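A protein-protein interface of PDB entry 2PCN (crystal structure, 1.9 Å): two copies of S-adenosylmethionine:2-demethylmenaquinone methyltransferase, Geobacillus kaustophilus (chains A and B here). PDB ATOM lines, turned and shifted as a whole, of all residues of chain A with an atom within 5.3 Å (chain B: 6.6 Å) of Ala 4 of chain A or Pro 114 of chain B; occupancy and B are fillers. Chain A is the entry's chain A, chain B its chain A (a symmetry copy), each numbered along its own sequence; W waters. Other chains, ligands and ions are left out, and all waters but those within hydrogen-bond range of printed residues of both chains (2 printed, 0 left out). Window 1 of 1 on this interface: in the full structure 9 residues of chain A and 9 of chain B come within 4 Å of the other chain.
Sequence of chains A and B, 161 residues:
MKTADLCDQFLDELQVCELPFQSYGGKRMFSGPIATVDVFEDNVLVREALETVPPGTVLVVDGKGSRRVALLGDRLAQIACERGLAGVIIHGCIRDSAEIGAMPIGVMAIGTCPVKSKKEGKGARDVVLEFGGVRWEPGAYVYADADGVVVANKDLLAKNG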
ATOM      1  N   LYS A   2       5.454   9.667  -2.776  1.00  0.00           N
ATOM      2  CA  LYS A   2       4.992   8.289  -2.907  1.00  0.00           C
ATOM      3  C   LYS A   2       4.125   8.196  -4.153  1.00  0.00           C
ATOM      4  O   LYS A   2       3.250   9.036  -4.366  1.00  0.00           O
ATOM      5  CB  LYS A   2       4.159   7.877  -1.688  1.00  0.00           C
ATOM      6  CG  LYS A   2       4.967   7.621  -0.427  1.00  0.00           C
ATOM      7  CD  LYS A   2       4.064   7.330   0.769  1.00  0.00           C
ATOM      8  CE  LYS A   2       3.023   6.251   0.461  1.00  0.00           C
ATOM      9  NZ  LYS A   2       3.630   4.949   0.048  1.00  0.00           N
ATOM     10  N   THR A   3       4.359   7.182  -4.978  1.00  0.00           N
ATOM     11  CA  THR A   3       3.563   7.018  -6.184  1.00  0.00           C
ATOM     12  C   THR A   3       2.113   6.732  -5.815  1.00  0.00           C
ATOM     13  O   THR A   3       1.198   7.087  -6.552  1.00  0.00           O
ATOM     14  CB  THR A   3       4.098   5.872  -7.069  1.00  0.00           C
ATOM     15  OG1 THR A   3       4.211   4.671  -6.291  1.00  0.00           O
ATOM     16  CG2 THR A   3       5.463   6.242  -7.636  1.00  0.00           C
ATOM     17  N   ALA A   4       1.908   6.100  -4.662  1.00  0.00           N
ATOM     18  CA  ALA A   4       0.561   5.782  -4.203  1.00  0.00           C
ATOM     19  C   ALA A   4      -0.221   7.067  -3.950  1.00  0.00           C
ATOM     20  O   ALA A   4      -1.383   7.179  -4.343  1.00  0.00           O
ATOM     21  CB  ALA A   4       0.628   4.948  -2.930  1.00  0.00           C
ATOM     22  N   ASP A   5       0.420   8.038  -3.301  1.00  0.00           N
ATOM     23  CA  ASP A   5      -0.235   9.311  -3.010  1.00  0.00           C
ATOM     24  C   ASP A   5      -0.486  10.117  -4.278  1.00  0.00           C
ATOM     25  O   ASP A   5      -1.523  10.766  -4.412  1.00  0.00           O
ATOM     26  CB  ASP A   5       0.601  10.147  -2.035  1.00  0.00           C
ATOM     27  CG  ASP A   5       0.662   9.538  -0.647  1.00  0.00           C
ATOM     28  OD1 ASP A   5      -0.316   8.875  -0.245  1.00  0.00           O
ATOM     29  OD2 ASP A   5       1.677   9.736   0.050  1.00  0.00           O
ATOM     30  N   LEU A   6       0.465  10.075  -5.207  1.00  0.00           N
ATOM     31  CA  LEU A   6       0.330  10.797  -6.469  1.00  0.00           C
ATOM     32  C   LEU A   6      -0.833  10.249  -7.287  1.00  0.00           C
ATOM     33  O   LEU A   6      -1.560  11.007  -7.934  1.00  0.00           O
ATOM     34  CB  LEU A   6       1.629  10.701  -7.270  1.00  0.00           C
ATOM     35  CG  LEU A   6       2.808  11.425  -6.620  1.00  0.00           C
ATOM     36  CD1 LEU A   6       4.095  11.121  -7.378  1.00  0.00           C
ATOM     37  CD2 LEU A   6       2.524  12.927  -6.599  1.00  0.00           C
ATOM     38  N   CYS A   7      -1.014   8.932  -7.266  1.00  0.00           N
ATOM     39  CA  CYS A   7      -2.116   8.341  -8.006  1.00  0.00           C
ATOM     40  C   CYS A   7      -3.452   8.754  -7.385  1.00  0.00           C
ATOM     41  O   CYS A   7      -4.399   9.070  -8.100  1.00  0.00           O
ATOM     42  CB  CYS A   7      -1.991   6.814  -8.042  1.00  0.00           C
ATOM     43  SG  CYS A   7      -0.716   6.200  -9.195  1.00  0.00           S
ATOM     44  N   ASP A   8      -3.524   8.771  -6.057  1.00  0.00           N
ATOM     45  CA  ASP A   8      -4.765   9.150  -5.379  1.00  0.00           C
ATOM     46  C   ASP A   8      -5.179  10.584  -5.703  1.00  0.00           C
ATOM     47  O   ASP A   8      -6.360  10.867  -5.889  1.00  0.00           O
ATOM     48  CB  ASP A   8      -4.625   9.003  -3.860  1.00  0.00           C
ATOM     49  CG  ASP A   8      -4.521   7.554  -3.415  1.00  0.00           C
ATOM     50  OD1 ASP A   8      -4.710   6.651  -4.257  1.00  0.00           O
ATOM     51  OD2 ASP A   8      -4.259   7.319  -2.215  1.00  0.00           O
ATOM     52  N   VAL A  16       0.644   5.356 -15.796  1.00  0.00           N
ATOM     53  CA  VAL A  16       1.214   4.397 -14.860  1.00  0.00           C
ATOM     54  C   VAL A  16       1.948   3.305 -15.624  1.00  0.00           C
ATOM     55  O   VAL A  16       1.351   2.587 -16.424  1.00  0.00           O
ATOM     56  CB  VAL A  16       0.115   3.760 -13.984  1.00  0.00           C
ATOM     57  CG1 VAL A  16       0.734   2.767 -13.014  1.00  0.00           C
ATOM     58  CG2 VAL A  16      -0.633   4.844 -13.222  1.00  0.00           C
ATOM     59  N   ASP A 145       9.234   4.790  -7.022  1.00  0.00           N
ATOM     60  CA  ASP A 145       9.457   4.296  -5.674  1.00  0.00           C
ATOM     61  C   ASP A 145       9.216   2.795  -5.634  1.00  0.00           C
ATOM     62  O   ASP A 145       9.054   2.159  -6.677  1.00  0.00           O
ATOM     63  CB  ASP A 145       8.592   5.040  -4.637  1.00  0.00           C
ATOM     64  CG  ASP A 145       7.114   4.730  -4.752  1.00  0.00           C
ATOM     65  OD1 ASP A 145       6.729   3.874  -5.574  1.00  0.00           O
ATOM     66  OD2 ASP A 145       6.333   5.351  -3.999  1.00  0.00           O
ATOM     67  N   ASP A 147       6.706   1.064  -5.001  1.00  0.00           N
ATOM     68  CA  ASP A 147       5.428   0.581  -5.526  1.00  0.00           C
ATOM     69  C   ASP A 147       5.280   0.652  -7.043  1.00  0.00           C
ATOM     70  O   ASP A 147       4.498  -0.096  -7.627  1.00  0.00           O
ATOM     71  CB  ASP A 147       4.266   1.331  -4.873  1.00  0.00           C
ATOM     72  CG  ASP A 147       4.173   1.063  -3.387  1.00  0.00           C
ATOM     73  OD1 ASP A 147       4.411  -0.094  -2.983  1.00  0.00           O
ATOM     74  OD2 ASP A 147       3.849   1.999  -2.628  1.00  0.00           O
ATOM     75  N   GLY A 148       6.023   1.546  -7.683  1.00  0.00           N
ATOM     76  CA  GLY A 148       5.914   1.653  -9.126  1.00  0.00           C
ATOM     77  C   GLY A 148       6.500   2.928  -9.693  1.00  0.00           C
ATOM     78  O   GLY A 148       7.282   3.616  -9.036  1.00  0.00           O
ATOM     79  N   VAL A 149       6.111   3.238 -10.925  1.00  0.00           N
ATOM     80  CA  VAL A 149       6.591   4.423 -11.620  1.00  0.00           C
ATOM     81  C   VAL A 149       5.432   5.103 -12.341  1.00  0.00           C
ATOM     82  O   VAL A 149       4.688   4.460 -13.078  1.00  0.00           O
ATOM     83  CB  VAL A 149       7.666   4.046 -12.663  1.00  0.00           C
ATOM     84  CG1 VAL A 149       8.137   5.294 -13.403  1.00  0.00           C
ATOM     85  CG2 VAL A 149       8.836   3.345 -11.977  1.00  0.00           C
ATOM     86  N   VAL A 150       5.282   6.405 -12.121  1.00  0.00           N
ATOM     87  CA  VAL A 150       4.220   7.170 -12.754  1.00  0.00           C
ATOM     88  C   VAL A 150       4.799   8.405 -13.432  1.00  0.00           C
ATOM     89  O   VAL A 150       5.778   8.985 -12.958  1.00  0.00           O
ATOM     90  CB  VAL A 150       3.141   7.593 -11.733  1.00  0.00           C
ATOM     91  CG1 VAL A 150       2.551   6.351 -11.075  1.00  0.00           C
ATOM     92  CG2 VAL A 150       3.732   8.526 -10.686  1.00  0.00           C
ATOM     93  N   ARG B  68      -3.624  -4.299 -12.129  1.00  0.00           N
ATOM     94  CA  ARG B  68      -4.097  -2.952 -12.431  1.00  0.00           C
ATOM     95  C   ARG B  68      -4.336  -2.081 -11.202  1.00  0.00           C
ATOM     96  O   ARG B  68      -4.325  -0.852 -11.297  1.00  0.00           O
ATOM     97  CB  ARG B  68      -5.367  -3.025 -13.286  1.00  0.00           C
ATOM     98  CG  ARG B  68      -5.149  -3.758 -14.605  1.00  0.00           C
ATOM     99  CD  ARG B  68      -6.267  -3.503 -15.609  1.00  0.00           C
ATOM    100  NE  ARG B  68      -7.570  -3.971 -15.145  1.00  0.00           N
ATOM    101  CZ  ARG B  68      -8.675  -3.947 -15.884  1.00  0.00           C
ATOM    102  NH1 ARG B  68      -8.636  -3.477 -17.124  1.00  0.00           N
ATOM    103  NH2 ARG B  68      -9.823  -4.387 -15.383  1.00  0.00           N
ATOM    104  N   VAL B  69      -4.553  -2.710 -10.050  1.00  0.00           N
ATOM    105  CA  VAL B  69      -4.768  -1.966  -8.813  1.00  0.00           C
ATOM    106  C   VAL B  69      -4.216  -2.721  -7.614  1.00  0.00           C
ATOM    107  O   VAL B  69      -3.972  -3.926  -7.679  1.00  0.00           O
ATOM    108  CB  VAL B  69      -6.276  -1.700  -8.535  1.00  0.00           C
ATOM    109  CG1 VAL B  69      -6.892  -0.896  -9.672  1.00  0.00           C
ATOM    110  CG2 VAL B  69      -7.012  -3.017  -8.345  1.00  0.00           C
ATOM    111  N   ALA B  70      -4.024  -1.997  -6.519  1.00  0.00           N
ATOM    112  CA  ALA B  70      -3.543  -2.591  -5.282  1.00  0.00           C
ATOM    113  C   ALA B  70      -4.788  -2.947  -4.471  1.00  0.00           C
ATOM    114  O   ALA B  70      -5.799  -2.246  -4.546  1.00  0.00           O
ATOM    115  CB  ALA B  70      -2.686  -1.588  -4.525  1.00  0.00           C
ATOM    116  N   ILE B  94      -0.333  -5.093  -4.063  1.00  0.00           N
ATOM    117  CA  ILE B  94      -0.458  -4.242  -2.889  1.00  0.00           C
ATOM    118  C   ILE B  94       0.307  -2.960  -3.198  1.00  0.00           C
ATOM    119  O   ILE B  94       0.944  -2.845  -4.249  1.00  0.00           O
ATOM    120  CB  ILE B  94       0.185  -4.881  -1.633  1.00  0.00           C
ATOM    121  CG1 ILE B  94       1.705  -4.982  -1.811  1.00  0.00           C
ATOM    122  CG2 ILE B  94      -0.410  -6.259  -1.387  1.00  0.00           C
ATOM    123  CD1 ILE B  94       2.449  -5.300  -0.532  1.00  0.00           C
ATOM    124  N   ARG B  95       0.224  -1.992  -2.292  1.00  0.00           N
ATOM    125  CA  ARG B  95       0.969  -0.751  -2.435  1.00  0.00           C
ATOM    126  C   ARG B  95       1.454  -0.377  -1.036  1.00  0.00           C
ATOM    127  O   ARG B  95       1.133  -1.073  -0.069  1.00  0.00           O
ATOM    128  CB  ARG B  95       0.115   0.354  -3.066  1.00  0.00           C
ATOM    129  CG  ARG B  95      -1.070   0.844  -2.257  1.00  0.00           C
ATOM    130  CD  ARG B  95      -1.785   1.930  -3.058  1.00  0.00           C
ATOM    131  NE  ARG B  95      -2.689   2.739  -2.247  1.00  0.00           N
ATOM    132  CZ  ARG B  95      -3.269   3.856  -2.672  1.00  0.00           C
ATOM    133  NH1 ARG B  95      -3.045   4.301  -3.904  1.00  0.00           N
ATOM    134  NH2 ARG B  95      -4.055   4.546  -1.856  1.00  0.00           N
ATOM    135  N   ASP B  96       2.217   0.706  -0.928  1.00  0.00           N
ATOM    136  CA  ASP B  96       2.796   1.130   0.347  1.00  0.00           C
ATOM    137  C   ASP B  96       3.690  -0.006   0.846  1.00  0.00           C
ATOM    138  O   ASP B  96       3.790  -0.249   2.051  1.00  0.00           O
ATOM    139  CB  ASP B  96       1.716   1.422   1.396  1.00  0.00           C
ATOM    140  CG  ASP B  96       0.770   2.532   0.975  1.00  0.00           C
ATOM    141  OD1 ASP B  96       1.239   3.544   0.412  1.00  0.00           O
ATOM    142  OD2 ASP B  96      -0.444   2.394   1.221  1.00  0.00           O
ATOM    143  N   THR B 112       3.394  -5.141  -6.929  1.00  0.00           N
ATOM    144  CA  THR B 112       2.958  -3.862  -6.388  1.00  0.00           C
ATOM    145  C   THR B 112       2.325  -3.040  -7.499  1.00  0.00           C
ATOM    146  O   THR B 112       2.643  -3.216  -8.673  1.00  0.00           O
ATOM    147  CB  THR B 112       4.135  -3.052  -5.802  1.00  0.00           C
ATOM    148  OG1 THR B 112       5.100  -2.787  -6.831  1.00  0.00           O
ATOM    149  CG2 THR B 112       4.799  -3.821  -4.663  1.00  0.00           C
ATOM    150  N   CYS B 113       1.421  -2.151  -7.108  1.00  0.00           N
ATOM    151  CA  CYS B 113       0.726  -1.265  -8.034  1.00  0.00           C
ATOM    152  C   CYS B 113       0.306  -0.054  -7.212  1.00  0.00           C
ATOM    153  O   CYS B 113      -0.361  -0.199  -6.190  1.00  0.00           O
ATOM    154  CB  CYS B 113      -0.511  -1.948  -8.609  1.00  0.00           C
ATOM    155  SG  CYS B 113      -1.460  -0.870  -9.702  1.00  0.00           S
ATOM    156  N   PRO B 114       0.691   1.155  -7.648  1.00  0.00           N
ATOM    157  CA  PRO B 114       0.350   2.385  -6.925  1.00  0.00           C
ATOM    158  C   PRO B 114      -1.105   2.840  -7.014  1.00  0.00           C
ATOM    159  O   PRO B 114      -1.546   3.663  -6.209  1.00  0.00           O
ATOM    160  CB  PRO B 114       1.306   3.407  -7.535  1.00  0.00           C
ATOM    161  CG  PRO B 114       1.341   2.976  -8.969  1.00  0.00           C
ATOM    162  CD  PRO B 114       1.484   1.462  -8.854  1.00  0.00           C
ATOM    163  N   VAL B 115      -1.853   2.302  -7.974  1.00  0.00           N
ATOM    164  CA  VAL B 115      -3.252   2.695  -8.154  1.00  0.00           C
ATOM    165  C   VAL B 115      -4.212   2.058  -7.149  1.00  0.00           C
ATOM    166  O   VAL B 115      -4.203   0.845  -6.946  1.00  0.00           O
ATOM    167  CB  VAL B 115      -3.746   2.348  -9.576  1.00  0.00           C
ATOM    168  CG1 VAL B 115      -5.184   2.819  -9.757  1.00  0.00           C
ATOM    169  CG2 VAL B 115      -2.831   2.988 -10.618  1.00  0.00           C
ATOM    170  N   LYS B 116      -5.051   2.884  -6.532  1.00  0.00           N
ATOM    171  CA  LYS B 116      -6.018   2.391  -5.551  1.00  0.00           C
ATOM    172  C   LYS B 116      -7.082   1.535  -6.234  1.00  0.00           C
ATOM    173  O   LYS B 116      -7.404   1.741  -7.406  1.00  0.00           O
ATOM    174  CB  LYS B 116      -6.685   3.568  -4.822  1.00  0.00           C
ATOM    175  CG  LYS B 116      -7.777   4.305  -5.607  1.00  0.00           C
ATOM    176  CD  LYS B 116      -7.394   4.542  -7.064  1.00  0.00           C
ATOM    177  CE  LYS B 116      -8.207   5.658  -7.700  1.00  0.00           C
ATOM    178  NZ  LYS B 116      -7.721   6.996  -7.256  1.00  0.00           N
HETATM  179  O   HOH W   1       3.536  -1.204 -10.783  1.00  0.00           O
HETATM  180  O   HOH W   2      -4.944   5.854  -7.019  1.00  0.00           O
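Among the printed residues, pairs that only touch across the chains: Thr 3 of chain A with Pro 114 of chain B, Ala 4 of chain A with Asp 96 of chain B, Ala 4 of chain A with Pro 114 of chain B, Cys 7 of chain A with Pro 114 of chain B, Asp 8 of chain A with Lys 116 of chain B, Val 16 of chain A with Val 115 of chain B, Asp 147 of chain A with Arg 95 of chain B, Asp 147 of chain A with Cys 113 of chain B and Asp 147 of chain A with Pro 114 of chain B.
Of the 13 printed residues of chain A, 7 touch a printed residue of chain B.
Printed residues of chain A that touch a printed residue of chain B: Lys 2, Thr 3, Ala 4, Cys 7, Asp 8, Val 16 and Asp 147.
Hydrophobic or aromatic side chains of chain A within 4 Å of the printed part of chain B: Ala 4 and Val 16.
Of the 11 printed residues of chain B, 7 touch a printed residue of chain A.
Printed residues of chain B that touch a printed residue of chain A: Arg 95, Asp 96, Thr 112, Cys 113, Pro 114, Val 115 and Lys 116.
Among the printed residues, 14 pairs touch across the chains.
Among the printed residues, Asp or Glu carboxylates within 4 Å of a Lys or Arg side-chain nitrogen of the other chain: Lys 2 of chain A with Asp 96 of chain B and Asp 8 of chain A with Arg 95 of chain B.
Ala 4 of chain A touches just these residues of chain B: Arg 95, Asp 96 and Pro 114.
Pro 114 of chain B touches just these residues of chain A: Thr 3 (3.4 Å), Ala 4 (3.6 Å), Cys 7 (3.7 Å) and Asp 147 (3.6 Å).
Of the printed residues of chain A, Val 115 of chain B touches Val 16 (3.9 Å).
Of the printed residues of chain B, Lys 2 of chain A touches Asp 96 (2.8 Å).
Of the printed residues of chain A, Arg 95 of chain B touches Ala 4, Asp 8 and Asp 147.
Of the printed residues of chain A, Asp 96 of chain B touches Lys 2 (2.8 Å), Ala 4 (3.7 Å) and Asp 147 (2.7 Å).
Val 69 of chain B touches none of the printed residues of chain A.
The nearest residue of chain B that does not touch Ala 4 of chain A is Val 115 of chain B (5.7 Å).
The nearest printed residue of chain B that does not touch Val 16 of chain A is Pro 114 of chain B (4.1 Å).
OD2 of Asp 147 of chain A is in salt-bridge range of NZ of Lys 2 of chain A, 3.99 Å away.
The backbone carbonyl oxygen (O) of Arg 68 of chain B is in hydrogen-bond range of the side-chain sulfur (SG) of Cys 113 of chain B.
The backbone carbonyl oxygen of Pro 114 of chain B sits at hydrogen-bond distance from the guanidinium group of Arg 95 of chain B (2.8 Å).
The backbone NH of Val 115 of chain B lies close to the side-chain sulfur of Cys 113 of chain B (3.6 Å).
The backbone NH (N) of Val 69 of chain B lies close to the side-chain sulfur (SG) of Cys 113 of chain B (3.6 Å).
The backbone carbonyl oxygen (O) of Ile 94 of chain B sits at hydrogen-bond distance from the backbone NH (N) of Cys 113 of chain B, 3.0 Å away.
The guanidinium group of Arg 95 of chain B is in hydrogen-bond range of the backbone carbonyl oxygen of Ala 4 of chain A (3.4 Å).
OD1 of Asp 96 of chain B lies within salt-bridge range of NZ of Lys 2 of chain A, 2.8 Å away.
The side-chain carboxylate (OD2) of Asp 8 of chain A is in salt-bridge range of the guanidinium group (NH2) of Arg 95 of chain B (2.8 Å).
N of Asp 96 of chain B is in hydrogen-bond range of OD2 of Asp 147 of chain A, 2.7 Å away.
The backbone carbonyl oxygen (O) of Asp 147 of chain A is in hydrogen-bond range of the side-chain hydroxyl (OG1) of Thr 112 of chain B (2.9 Å).
No position is printed for both chains.
Of the 14 pairs that touch across the chains among the printed residues, none has its exchanged pair printed and touching as well.
Water W2 lies within hydrogen-bond range of the side-chain carboxylate of Asp 8 of chain A (2.9 Å), the backbone NH of Lys 116 of chain B (3.0 Å) and the backbone carbonyl oxygen of Cys 7 of chain A (3.4 Å).
Water W1 lies within hydrogen-bond range of the backbone carbonyl oxygen of Thr 112 of chain B and the backbone carbonyl oxygen of Asp 147 of chain A.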
